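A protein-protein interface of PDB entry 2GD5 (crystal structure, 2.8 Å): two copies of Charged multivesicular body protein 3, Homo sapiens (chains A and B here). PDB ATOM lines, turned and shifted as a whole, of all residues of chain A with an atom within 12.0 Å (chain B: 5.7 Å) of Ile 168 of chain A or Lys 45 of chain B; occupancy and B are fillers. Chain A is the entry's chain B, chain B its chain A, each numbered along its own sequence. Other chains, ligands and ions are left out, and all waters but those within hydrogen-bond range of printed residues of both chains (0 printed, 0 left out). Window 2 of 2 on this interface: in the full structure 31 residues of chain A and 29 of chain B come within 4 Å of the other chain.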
ATOM      1  N   ALA A  92       9.665 -12.757 -36.485  1.00  0.00           N
ATOM      2  CA  ALA A  92       9.499 -11.802 -35.397  1.00  0.00           C
ATOM      3  C   ALA A  92       8.033 -11.693 -34.987  1.00  0.00           C
ATOM      4  O   ALA A  92       7.674 -11.945 -33.839  1.00  0.00           O
ATOM      5  CB  ALA A  92      10.023 -10.459 -35.798  1.00  0.00           C
ATOM      6  N   VAL A  93       7.183 -11.348 -35.938  1.00  0.00           N
ATOM      7  CA  VAL A  93       5.772 -11.223 -35.662  1.00  0.00           C
ATOM      8  C   VAL A  93       5.227 -12.472 -34.998  1.00  0.00           C
ATOM      9  O   VAL A  93       4.345 -12.375 -34.164  1.00  0.00           O
ATOM     10  CB  VAL A  93       4.981 -10.970 -36.930  1.00  0.00           C
ATOM     11  CG1 VAL A  93       3.552 -10.711 -36.588  1.00  0.00           C
ATOM     12  CG2 VAL A  93       5.551  -9.768 -37.681  1.00  0.00           C
ATOM     13  N   LEU A  94       5.756 -13.642 -35.351  1.00  0.00           N
ATOM     14  CA  LEU A  94       5.271 -14.921 -34.780  1.00  0.00           C
ATOM     15  C   LEU A  94       5.741 -15.177 -33.356  1.00  0.00           C
ATOM     16  O   LEU A  94       5.024 -15.745 -32.546  1.00  0.00           O
ATOM     17  CB  LEU A  94       5.707 -16.084 -35.664  1.00  0.00           C
ATOM     18  CG  LEU A  94       4.665 -16.735 -36.571  1.00  0.00           C
ATOM     19  CD1 LEU A  94       5.303 -17.069 -37.900  1.00  0.00           C
ATOM     20  CD2 LEU A  94       4.151 -17.982 -35.874  1.00  0.00           C
ATOM     21  N   ARG A  95       6.969 -14.747 -33.088  1.00  0.00           N
ATOM     22  CA  ARG A  95       7.638 -14.878 -31.807  1.00  0.00           C
ATOM     23  C   ARG A  95       6.735 -14.390 -30.697  1.00  0.00           C
ATOM     24  O   ARG A  95       6.749 -14.961 -29.612  1.00  0.00           O
ATOM     25  CB  ARG A  95       8.943 -14.075 -31.838  1.00  0.00           C
ATOM     26  CG  ARG A  95       9.980 -14.462 -30.781  1.00  0.00           C
ATOM     27  CD  ARG A  95       9.965 -13.514 -29.536  1.00  0.00           C
ATOM     28  NE  ARG A  95      11.085 -12.550 -29.470  1.00  0.00           N
ATOM     29  CZ  ARG A  95      10.993 -11.320 -28.957  1.00  0.00           C
ATOM     30  NH1 ARG A  95       9.840 -10.875 -28.489  1.00  0.00           N
ATOM     31  NH2 ARG A  95      12.052 -10.528 -28.915  1.00  0.00           N
ATOM     32  N   VAL A  96       5.931 -13.358 -30.971  1.00  0.00           N
ATOM     33  CA  VAL A  96       5.006 -12.790 -29.955  1.00  0.00           C
ATOM     34  C   VAL A  96       3.505 -13.030 -30.250  1.00  0.00           C
ATOM     35  O   VAL A  96       2.676 -13.080 -29.341  1.00  0.00           O
ATOM     36  CB  VAL A  96       5.268 -11.251 -29.677  1.00  0.00           C
ATOM     37  CG1 VAL A  96       6.770 -10.947 -29.472  1.00  0.00           C
ATOM     38  CG2 VAL A  96       4.679 -10.360 -30.782  1.00  0.00           C
ATOM     39  N   ALA A  97       3.154 -13.161 -31.521  1.00  0.00           N
ATOM     40  CA  ALA A  97       1.787 -13.479 -31.865  1.00  0.00           C
ATOM     41  C   ALA A  97       1.694 -14.979 -31.982  1.00  0.00           C
ATOM     42  O   ALA A  97       1.101 -15.637 -31.113  1.00  0.00           O
ATOM     43  CB  ALA A  97       1.388 -12.833 -33.163  1.00  0.00           C
ATOM     44  N   GLY A  98       2.309 -15.519 -33.036  1.00  0.00           N
ATOM     45  CA  GLY A  98       2.120 -16.917 -33.394  1.00  0.00           C
ATOM     46  C   GLY A  98       1.140 -17.025 -34.556  1.00  0.00           C
ATOM     47  O   GLY A  98       0.281 -17.931 -34.599  1.00  0.00           O
ATOM     48  N   SER A  99       1.264 -16.095 -35.504  1.00  0.00           N
ATOM     49  CA  SER A  99       0.433 -16.116 -36.701  1.00  0.00           C
ATOM     50  C   SER A  99       0.934 -15.082 -37.692  1.00  0.00           C
ATOM     51  O   SER A  99       1.022 -13.896 -37.357  1.00  0.00           O
ATOM     52  CB  SER A  99      -1.026 -15.813 -36.344  1.00  0.00           C
ATOM     53  OG  SER A  99      -1.138 -14.497 -35.820  1.00  0.00           O
ATOM     54  N   LEU A 100       1.236 -15.527 -38.910  1.00  0.00           N
ATOM     55  CA  LEU A 100       1.711 -14.638 -39.975  1.00  0.00           C
ATOM     56  C   LEU A 100       0.756 -13.488 -40.177  1.00  0.00           C
ATOM     57  O   LEU A 100      -0.237 -13.404 -39.481  1.00  0.00           O
ATOM     58  CB  LEU A 100       1.886 -15.411 -41.290  1.00  0.00           C
ATOM     59  CG  LEU A 100       2.885 -16.552 -41.186  1.00  0.00           C
ATOM     60  CD1 LEU A 100       2.893 -17.292 -42.472  1.00  0.00           C
ATOM     61  CD2 LEU A 100       4.269 -16.034 -40.853  1.00  0.00           C
ATOM     62  N   MET A 159      -9.240  -4.259 -37.082  1.00  0.00           N
ATOM     63  CA  MET A 159      -9.678  -5.113 -36.004  1.00  0.00           C
ATOM     64  C   MET A 159      -8.384  -5.614 -35.432  1.00  0.00           C
ATOM     65  O   MET A 159      -8.342  -6.640 -34.759  1.00  0.00           O
ATOM     66  CB  MET A 159     -10.467  -6.295 -36.543  1.00  0.00           C
ATOM     67  CG  MET A 159     -11.339  -6.935 -35.482  1.00  0.00           C
ATOM     68  SD  MET A 159     -11.646  -8.816 -35.752  1.00  0.00           S
ATOM     69  CE  MET A 159      -9.939  -9.494 -35.211  1.00  0.00           C
ATOM     70  N   GLU A 160      -7.315  -4.888 -35.736  1.00  0.00           N
ATOM     71  CA  GLU A 160      -5.976  -5.298 -35.371  1.00  0.00           C
ATOM     72  C   GLU A 160      -5.856  -5.715 -33.913  1.00  0.00           C
ATOM     73  O   GLU A 160      -5.487  -6.853 -33.623  1.00  0.00           O
ATOM     74  CB  GLU A 160      -4.982  -4.192 -35.713  1.00  0.00           C
ATOM     75  CG  GLU A 160      -4.206  -4.439 -37.027  1.00  0.00           C
ATOM     76  CD  GLU A 160      -3.031  -5.408 -36.854  1.00  0.00           C
ATOM     77  OE1 GLU A 160      -3.220  -6.471 -36.189  1.00  0.00           O
ATOM     78  OE2 GLU A 160      -1.929  -5.101 -37.390  1.00  0.00           O
ATOM     79  N   ILE A 161      -6.191  -4.796 -33.013  1.00  0.00           N
ATOM     80  CA  ILE A 161      -6.170  -5.017 -31.563  1.00  0.00           C
ATOM     81  C   ILE A 161      -6.955  -6.248 -31.091  1.00  0.00           C
ATOM     82  O   ILE A 161      -6.463  -7.043 -30.298  1.00  0.00           O
ATOM     83  CB  ILE A 161      -6.666  -3.766 -30.794  1.00  0.00           C
ATOM     84  CG1 ILE A 161      -8.177  -3.592 -30.926  1.00  0.00           C
ATOM     85  CG2 ILE A 161      -5.917  -2.519 -31.236  1.00  0.00           C
ATOM     86  CD1 ILE A 161      -8.736  -3.596 -32.355  1.00  0.00           C
ATOM     87  N   ASP A 162      -8.174  -6.419 -31.572  1.00  0.00           N
ATOM     88  CA  ASP A 162      -8.915  -7.592 -31.199  1.00  0.00           C
ATOM     89  C   ASP A 162      -8.139  -8.871 -31.576  1.00  0.00           C
ATOM     90  O   ASP A 162      -7.928  -9.766 -30.739  1.00  0.00           O
ATOM     91  CB  ASP A 162     -10.303  -7.540 -31.815  1.00  0.00           C
ATOM     92  CG  ASP A 162     -11.258  -6.700 -31.000  1.00  0.00           C
ATOM     93  OD1 ASP A 162     -11.126  -6.697 -29.754  1.00  0.00           O
ATOM     94  OD2 ASP A 162     -12.134  -6.034 -31.606  1.00  0.00           O
ATOM     95  N   ARG A 163      -7.682  -8.938 -32.822  1.00  0.00           N
ATOM     96  CA  ARG A 163      -6.966 -10.112 -33.275  1.00  0.00           C
ATOM     97  C   ARG A 163      -5.734 -10.261 -32.396  1.00  0.00           C
ATOM     98  O   ARG A 163      -5.327 -11.383 -32.040  1.00  0.00           O
ATOM     99  CB  ARG A 163      -6.597  -9.991 -34.757  1.00  0.00           C
ATOM    100  CG  ARG A 163      -5.835 -11.179 -35.305  1.00  0.00           C
ATOM    101  CD  ARG A 163      -5.534 -11.076 -36.829  1.00  0.00           C
ATOM    102  NE  ARG A 163      -4.683  -9.951 -37.219  1.00  0.00           N
ATOM    103  CZ  ARG A 163      -5.141  -8.796 -37.705  1.00  0.00           C
ATOM    104  NH1 ARG A 163      -6.452  -8.586 -37.876  1.00  0.00           N
ATOM    105  NH2 ARG A 163      -4.286  -7.836 -38.020  1.00  0.00           N
ATOM    106  N   ILE A 164      -5.177  -9.110 -32.015  1.00  0.00           N
ATOM    107  CA  ILE A 164      -3.960  -9.055 -31.212  1.00  0.00           C
ATOM    108  C   ILE A 164      -4.195  -9.564 -29.799  1.00  0.00           C
ATOM    109  O   ILE A 164      -3.422 -10.388 -29.307  1.00  0.00           O
ATOM    110  CB  ILE A 164      -3.413  -7.620 -31.166  1.00  0.00           C
ATOM    111  CG1 ILE A 164      -2.764  -7.293 -32.494  1.00  0.00           C
ATOM    112  CG2 ILE A 164      -2.392  -7.454 -30.071  1.00  0.00           C
ATOM    113  CD1 ILE A 164      -2.542  -5.810 -32.683  1.00  0.00           C
ATOM    114  N   LEU A 165      -5.254  -9.063 -29.159  1.00  0.00           N
ATOM    115  CA  LEU A 165      -5.533  -9.412 -27.785  1.00  0.00           C
ATOM    116  C   LEU A 165      -5.830 -10.870 -27.742  1.00  0.00           C
ATOM    117  O   LEU A 165      -5.461 -11.571 -26.804  1.00  0.00           O
ATOM    118  CB  LEU A 165      -6.757  -8.702 -27.293  1.00  0.00           C
ATOM    119  CG  LEU A 165      -6.683  -7.205 -27.184  1.00  0.00           C
ATOM    120  CD1 LEU A 165      -8.092  -6.729 -27.199  1.00  0.00           C
ATOM    121  CD2 LEU A 165      -5.964  -6.787 -25.925  1.00  0.00           C
ATOM    122  N   PHE A 166      -6.527 -11.313 -28.784  1.00  0.00           N
ATOM    123  CA  PHE A 166      -6.894 -12.694 -28.911  1.00  0.00           C
ATOM    124  C   PHE A 166      -5.613 -13.499 -29.081  1.00  0.00           C
ATOM    125  O   PHE A 166      -5.391 -14.453 -28.341  1.00  0.00           O
ATOM    126  CB  PHE A 166      -7.820 -12.851 -30.084  1.00  0.00           C
ATOM    127  CG  PHE A 166      -8.373 -14.223 -30.241  1.00  0.00           C
ATOM    128  CD1 PHE A 166      -7.545 -15.292 -30.614  1.00  0.00           C
ATOM    129  CD2 PHE A 166      -9.720 -14.449 -30.073  1.00  0.00           C
ATOM    130  CE1 PHE A 166      -8.068 -16.578 -30.784  1.00  0.00           C
ATOM    131  CE2 PHE A 166     -10.241 -15.707 -30.238  1.00  0.00           C
ATOM    132  CZ  PHE A 166      -9.428 -16.774 -30.593  1.00  0.00           C
ATOM    133  N   GLU A 167      -4.739 -13.089 -29.996  1.00  0.00           N
ATOM    134  CA  GLU A 167      -3.431 -13.758 -30.125  1.00  0.00           C
ATOM    135  C   GLU A 167      -2.707 -13.844 -28.767  1.00  0.00           C
ATOM    136  O   GLU A 167      -2.467 -14.915 -28.254  1.00  0.00           O
ATOM    137  CB  GLU A 167      -2.568 -13.103 -31.233  1.00  0.00           C
ATOM    138  CG  GLU A 167      -3.013 -13.502 -32.667  1.00  0.00           C
ATOM    139  CD  GLU A 167      -2.660 -12.503 -33.815  1.00  0.00           C
ATOM    140  OE1 GLU A 167      -3.162 -12.755 -34.955  1.00  0.00           O
ATOM    141  OE2 GLU A 167      -1.889 -11.505 -33.610  1.00  0.00           O
ATOM    142  N   ILE A 168      -2.441 -12.716 -28.141  1.00  0.00           N
ATOM    143  CA  ILE A 168      -1.649 -12.715 -26.929  1.00  0.00           C
ATOM    144  C   ILE A 168      -2.271 -13.400 -25.713  1.00  0.00           C
ATOM    145  O   ILE A 168      -1.557 -13.861 -24.826  1.00  0.00           O
ATOM    146  CB  ILE A 168      -1.298 -11.303 -26.560  1.00  0.00           C
ATOM    147  CG1 ILE A 168      -0.438 -10.700 -27.665  1.00  0.00           C
ATOM    148  CG2 ILE A 168      -0.553 -11.316 -25.276  1.00  0.00           C
ATOM    149  CD1 ILE A 168      -0.500  -9.230 -27.744  1.00  0.00           C
ATOM    150  N   THR A 169      -3.596 -13.467 -25.659  1.00  0.00           N
ATOM    151  CA  THR A 169      -4.274 -13.982 -24.467  1.00  0.00           C
ATOM    152  C   THR A 169      -4.935 -15.326 -24.701  1.00  0.00           C
ATOM    153  O   THR A 169      -5.769 -15.752 -23.897  1.00  0.00           O
ATOM    154  CB  THR A 169      -5.339 -12.998 -23.966  1.00  0.00           C
ATOM    155  OG1 THR A 169      -6.419 -12.981 -24.901  1.00  0.00           O
ATOM    156  CG2 THR A 169      -4.734 -11.594 -23.825  1.00  0.00           C
ATOM    157  N   ALA A 170      -4.560 -15.984 -25.800  1.00  0.00           N
ATOM    158  CA  ALA A 170      -5.029 -17.339 -26.094  1.00  0.00           C
ATOM    159  C   ALA A 170      -6.567 -17.393 -26.203  1.00  0.00           C
ATOM    160  O   ALA A 170      -7.237 -18.238 -25.573  1.00  0.00           O
ATOM    161  CB  ALA A 170      -4.526 -18.303 -25.039  1.00  0.00           C
ATOM    162  N   GLY A 171      -7.117 -16.472 -26.995  1.00  0.00           N
ATOM    163  CA  GLY A 171      -8.555 -16.354 -27.181  1.00  0.00           C
ATOM    164  C   GLY A 171      -9.371 -16.080 -25.929  1.00  0.00           C
ATOM    165  O   GLY A 171     -10.396 -16.689 -25.746  1.00  0.00           O
ATOM    166  N   ALA A 172      -8.927 -15.178 -25.061  1.00  0.00           N
ATOM    167  CA  ALA A 172      -9.722 -14.813 -23.899  1.00  0.00           C
ATOM    168  C   ALA A 172     -10.353 -13.426 -23.996  1.00  0.00           C
ATOM    169  O   ALA A 172     -11.443 -13.232 -23.484  1.00  0.00           O
ATOM    170  CB  ALA A 172      -8.933 -14.951 -22.622  1.00  0.00           C
ATOM    171  N   LEU A 173      -9.668 -12.468 -24.618  1.00  0.00           N
ATOM    172  CA  LEU A 173     -10.262 -11.161 -24.908  1.00  0.00           C
ATOM    173  C   LEU A 173     -10.357 -11.095 -26.396  1.00  0.00           C
ATOM    174  O   LEU A 173      -9.607 -10.444 -27.090  1.00  0.00           O
ATOM    175  CB  LEU A 173      -9.466 -10.003 -24.329  1.00  0.00           C
ATOM    176  CG  LEU A 173      -9.504  -9.862 -22.798  1.00  0.00           C
ATOM    177  CD1 LEU A 173      -8.653  -8.688 -22.394  1.00  0.00           C
ATOM    178  CD2 LEU A 173     -10.912  -9.698 -22.239  1.00  0.00           C
ATOM    179  N   GLY A 174     -11.352 -11.830 -26.850  1.00  0.00           N
ATOM    180  CA  GLY A 174     -11.501 -12.239 -28.227  1.00  0.00           C
ATOM    181  C   GLY A 174     -11.494 -11.132 -29.207  1.00  0.00           C
ATOM    182  O   GLY A 174     -11.129 -10.021 -28.893  1.00  0.00           O
ATOM    183  N   LYS A 175     -11.895 -11.486 -30.410  1.00  0.00           N
ATOM    184  CA  LYS A 175     -11.951 -10.569 -31.495  1.00  0.00           C
ATOM    185  C   LYS A 175     -13.386 -10.014 -31.639  1.00  0.00           C
ATOM    186  O   LYS A 175     -14.320 -10.544 -31.028  1.00  0.00           O
ATOM    187  CB  LYS A 175     -11.428 -11.276 -32.734  1.00  0.00           C
ATOM    188  CG  LYS A 175     -11.270 -12.794 -32.600  1.00  0.00           C
ATOM    189  CD  LYS A 175     -10.813 -13.379 -33.940  1.00  0.00           C
ATOM    190  CE  LYS A 175     -11.438 -14.730 -34.215  1.00  0.00           C
ATOM    191  NZ  LYS A 175     -11.394 -14.986 -35.679  1.00  0.00           N
ATOM    192  N   VAL B  40       5.541  -5.751 -22.865  1.00  0.00           N
ATOM    193  CA  VAL B  40       4.202  -5.289 -23.177  1.00  0.00           C
ATOM    194  C   VAL B  40       3.246  -6.454 -23.293  1.00  0.00           C
ATOM    195  O   VAL B  40       2.166  -6.400 -22.756  1.00  0.00           O
ATOM    196  CB  VAL B  40       4.190  -4.483 -24.463  1.00  0.00           C
ATOM    197  CG1 VAL B  40       2.799  -3.926 -24.743  1.00  0.00           C
ATOM    198  CG2 VAL B  40       5.244  -3.369 -24.371  1.00  0.00           C
ATOM    199  N   LYS B  41       3.658  -7.515 -23.980  1.00  0.00           N
ATOM    200  CA  LYS B  41       2.846  -8.740 -24.106  1.00  0.00           C
ATOM    201  C   LYS B  41       2.423  -9.357 -22.760  1.00  0.00           C
ATOM    202  O   LYS B  41       1.295  -9.853 -22.642  1.00  0.00           O
ATOM    203  CB  LYS B  41       3.564  -9.754 -24.980  1.00  0.00           C
ATOM    204  CG  LYS B  41       3.112 -11.156 -24.770  1.00  0.00           C
ATOM    205  CD  LYS B  41       3.829 -12.150 -25.692  1.00  0.00           C
ATOM    206  CE  LYS B  41       3.220 -13.559 -25.545  1.00  0.00           C
ATOM    207  NZ  LYS B  41       4.199 -14.631 -25.921  1.00  0.00           N
ATOM    208  N   ARG B  42       3.315  -9.287 -21.754  1.00  0.00           N
ATOM    209  CA  ARG B  42       3.033  -9.763 -20.380  1.00  0.00           C
ATOM    210  C   ARG B  42       2.073  -8.822 -19.702  1.00  0.00           C
ATOM    211  O   ARG B  42       1.167  -9.247 -19.011  1.00  0.00           O
ATOM    212  CB  ARG B  42       4.289  -9.844 -19.507  1.00  0.00           C
ATOM    213  CG  ARG B  42       5.472 -10.618 -20.061  1.00  0.00           C
ATOM    214  CD  ARG B  42       6.667 -10.479 -19.090  1.00  0.00           C
ATOM    215  NE  ARG B  42       7.960 -10.298 -19.775  1.00  0.00           N
ATOM    216  CZ  ARG B  42       8.811 -11.287 -20.054  1.00  0.00           C
ATOM    217  NH1 ARG B  42       8.519 -12.541 -19.709  1.00  0.00           N
ATOM    218  NH2 ARG B  42       9.962 -11.028 -20.671  1.00  0.00           N
ATOM    219  N   SER B  43       2.284  -7.530 -19.895  1.00  0.00           N
ATOM    220  CA  SER B  43       1.363  -6.546 -19.358  1.00  0.00           C
ATOM    221  C   SER B  43      -0.066  -6.799 -19.857  1.00  0.00           C
ATOM    222  O   SER B  43      -1.028  -6.777 -19.069  1.00  0.00           O
ATOM    223  CB  SER B  43       1.810  -5.126 -19.721  1.00  0.00           C
ATOM    224  OG  SER B  43       3.170  -4.917 -19.398  1.00  0.00           O
ATOM    225  N   VAL B  44      -0.179  -7.043 -21.161  1.00  0.00           N
ATOM    226  CA  VAL B  44      -1.448  -7.304 -21.806  1.00  0.00           C
ATOM    227  C   VAL B  44      -2.116  -8.534 -21.209  1.00  0.00           C
ATOM    228  O   VAL B  44      -3.358  -8.583 -21.077  1.00  0.00           O
ATOM    229  CB  VAL B  44      -1.292  -7.496 -23.308  1.00  0.00           C
ATOM    230  CG1 VAL B  44      -2.628  -7.848 -23.920  1.00  0.00           C
ATOM    231  CG2 VAL B  44      -0.806  -6.240 -23.943  1.00  0.00           C
ATOM    232  N   LYS B  45      -1.294  -9.511 -20.826  1.00  0.00           N
ATOM    233  CA  LYS B  45      -1.827 -10.713 -20.216  1.00  0.00           C
ATOM    234  C   LYS B  45      -2.415 -10.431 -18.847  1.00  0.00           C
ATOM    235  O   LYS B  45      -3.575 -10.753 -18.599  1.00  0.00           O
ATOM    236  CB  LYS B  45      -0.768 -11.799 -20.162  1.00  0.00           C
ATOM    237  CG  LYS B  45      -0.334 -12.242 -21.537  1.00  0.00           C
ATOM    238  CD  LYS B  45      -0.187 -13.720 -21.602  1.00  0.00           C
ATOM    239  CE  LYS B  45       0.657 -14.072 -22.784  1.00  0.00           C
ATOM    240  NZ  LYS B  45       1.195 -15.434 -22.560  1.00  0.00           N
ATOM    241  N   ASP B  46      -1.627  -9.813 -17.967  1.00  0.00           N
ATOM    242  CA  ASP B  46      -2.096  -9.441 -16.631  1.00  0.00           C
ATOM    243  C   ASP B  46      -3.318  -8.585 -16.728  1.00  0.00           C
ATOM    244  O   ASP B  46      -4.323  -8.894 -16.097  1.00  0.00           O
ATOM    245  CB  ASP B  46      -1.026  -8.671 -15.858  1.00  0.00           C
ATOM    246  CG  ASP B  46      -0.036  -9.584 -15.186  1.00  0.00           C
ATOM    247  OD1 ASP B  46      -0.378 -10.097 -14.084  1.00  0.00           O
ATOM    248  OD2 ASP B  46       1.069  -9.794 -15.767  1.00  0.00           O
ATOM    249  N   ALA B  47      -3.234  -7.512 -17.516  1.00  0.00           N
ATOM    250  CA  ALA B  47      -4.353  -6.582 -17.662  1.00  0.00           C
ATOM    251  C   ALA B  47      -5.613  -7.317 -18.048  1.00  0.00           C
ATOM    252  O   ALA B  47      -6.670  -7.072 -17.465  1.00  0.00           O
ATOM    253  CB  ALA B  47      -4.057  -5.525 -18.676  1.00  0.00           C
ATOM    254  N   ALA B  48      -5.504  -8.229 -19.011  1.00  0.00           N
ATOM    255  CA  ALA B  48      -6.636  -9.083 -19.351  1.00  0.00           C
ATOM    256  C   ALA B  48      -7.154  -9.947 -18.197  1.00  0.00           C
ATOM    257  O   ALA B  48      -8.366 -10.021 -17.970  1.00  0.00           O
ATOM    258  CB  ALA B  48      -6.315  -9.921 -20.516  1.00  0.00           C
ATOM    259  N   LYS B  49      -6.258 -10.589 -17.456  1.00  0.00           N
ATOM    260  CA  LYS B  49      -6.696 -11.399 -16.321  1.00  0.00           C
ATOM    261  C   LYS B  49      -7.418 -10.589 -15.283  1.00  0.00           C
ATOM    262  O   LYS B  49      -8.374 -11.070 -14.709  1.00  0.00           O
ATOM    263  CB  LYS B  49      -5.550 -12.188 -15.673  1.00  0.00           C
ATOM    264  CG  LYS B  49      -5.341 -13.538 -16.357  1.00  0.00           C
ATOM    265  CD  LYS B  49      -4.494 -14.539 -15.572  1.00  0.00           C
ATOM    266  CE  LYS B  49      -4.049 -15.675 -16.511  1.00  0.00           C
ATOM    267  NZ  LYS B  49      -3.200 -15.111 -17.630  1.00  0.00           N
ATOM    268  N   LYS B  50      -6.974  -9.358 -15.046  1.00  0.00           N
ATOM    269  CA  LYS B  50      -7.618  -8.535 -14.024  1.00  0.00           C
ATOM    270  C   LYS B  50      -8.796  -7.797 -14.623  1.00  0.00           C
ATOM    271  O   LYS B  50      -9.406  -6.959 -13.971  1.00  0.00           O
ATOM    272  CB  LYS B  50      -6.642  -7.553 -13.383  1.00  0.00           C
ATOM    273  CG  LYS B  50      -5.433  -8.184 -12.752  1.00  0.00           C
ATOM    274  CD  LYS B  50      -4.421  -7.087 -12.447  1.00  0.00           C
ATOM    275  CE  LYS B  50      -3.025  -7.611 -12.083  1.00  0.00           C
ATOM    276  NZ  LYS B  50      -3.048  -8.383 -10.815  1.00  0.00           N
ATOM    277  N   MET B  63       1.534  -2.394 -29.230  1.00  0.00           N
ATOM    278  CA  MET B  63       2.086  -3.470 -30.011  1.00  0.00           C
ATOM    279  C   MET B  63       1.980  -3.149 -31.464  1.00  0.00           C
ATOM    280  O   MET B  63       3.000  -3.154 -32.136  1.00  0.00           O
ATOM    281  CB  MET B  63       1.343  -4.731 -29.730  1.00  0.00           C
ATOM    282  CG  MET B  63       1.305  -5.084 -28.295  1.00  0.00           C
ATOM    283  SD  MET B  63       2.668  -6.355 -27.824  1.00  0.00           S
ATOM    284  CE  MET B  63       1.579  -7.147 -26.451  1.00  0.00           C
ATOM    285  N   ARG B  67       5.136  -3.373 -33.938  1.00  0.00           N
ATOM    286  CA  ARG B  67       5.308  -4.157 -35.151  1.00  0.00           C
ATOM    287  C   ARG B  67       5.567  -3.251 -36.342  1.00  0.00           C
ATOM    288  O   ARG B  67       6.575  -3.428 -37.052  1.00  0.00           O
ATOM    289  CB  ARG B  67       4.118  -5.066 -35.400  1.00  0.00           C
ATOM    290  CG  ARG B  67       4.054  -6.234 -34.439  1.00  0.00           C
ATOM    291  CD  ARG B  67       2.803  -7.109 -34.736  1.00  0.00           C
ATOM    292  NE  ARG B  67       2.545  -8.106 -33.680  1.00  0.00           N
ATOM    293  CZ  ARG B  67       1.629  -9.073 -33.758  1.00  0.00           C
ATOM    294  NH1 ARG B  67       0.858  -9.185 -34.843  1.00  0.00           N
ATOM    295  NH2 ARG B  67       1.465  -9.907 -32.728  1.00  0.00           N
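Of the printed residues of chain B, Val 93 of chain A touches Arg 67. Leu 94 of chain A touches none of the printed residues of chain B. Of the printed residues of chain B, Val 96 of chain A touches Lys 41 and Arg 67. Printed residues of chain B within 4 Å of Glu 167 of chain A: Arg 67 (3.8 Å). Ile 168 of chain A touches just these residues of chain B: Lys 41 (3.5 Å), Lys 45 (3.0 Å) and Met 63 (3.2 Å). Of the printed residues of chain A, Lys 41 of chain B touches Val 96 and Ile 168. No residue of chain A comes within 4 Å of Val 44 of chain B. Lys 45 of chain B touches just one residue of chain A: Ile 168. No residue of chain A comes within 4 Å of Asp 46 of chain B. Of the printed residues of chain A, Ala 48 of chain B touches Leu 173. No residue of chain A comes within 4 Å of Lys 49 of chain B. Lys 50 of chain B touches none of the printed residues of chain A. Of the printed residues of chain A, Met 63 of chain B touches Ile 168 (3.2 Å). Of the printed residues of chain A, Arg 67 of chain B touches Val 93, Val 96, Ala 97 and Glu 167. The nearest printed residue of chain B that does not touch Leu 173 of chain A is Val 44 of chain B (5.5 Å).
Among the printed residues, merely in contact across the chains: Val 93 of chain A with Arg 67 of chain B (3.6 Å), Val 96 of chain A with Lys 41 of chain B (3.9 Å), Val 96 of chain A with Arg 67 of chain B (3.8 Å), Ala 97 of chain A with Arg 67 of chain B (3.0 Å), Ile 168 of chain A with Lys 41 of chain B (3.5 Å), Ile 168 of chain A with Lys 45 of chain B (3.0 Å), Ile 168 of chain A with Met 63 of chain B (3.2 Å) and Leu 173 of chain A with Ala 48 of chain B (3.2 Å).
Of the 26 printed residues of chain A, 6 touch a printed residue of chain B. Among the printed residues, 9 pairs touch across the chains.
The backbone NH (N) of Leu 173 of chain A lies within hydrogen-bond range of the side-chain hydroxyl (OG1) of Thr 169 of chain A (3.3 Å). The guanidinium group of Arg 163 of chain A lies within salt-bridge range of the side-chain carboxylate of Glu 167 of chain A (3.9 Å). The side-chain carboxylate (OE1) of Glu 167 of chain A is in hydrogen-bond range of the side-chain hydroxyl (OG) of Ser 99 of chain A, 2.8 Å away.
The guanidinium group (NH1) of Arg 67 of chain B is in salt-bridge range of the side-chain carboxylate (OE2) of Glu 167 of chain A, at 3.8 Å.
No position is printed for both chains. Of the 9 pairs that touch across the chains among the printed residues, none has its exchanged pair printed and touching as well.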
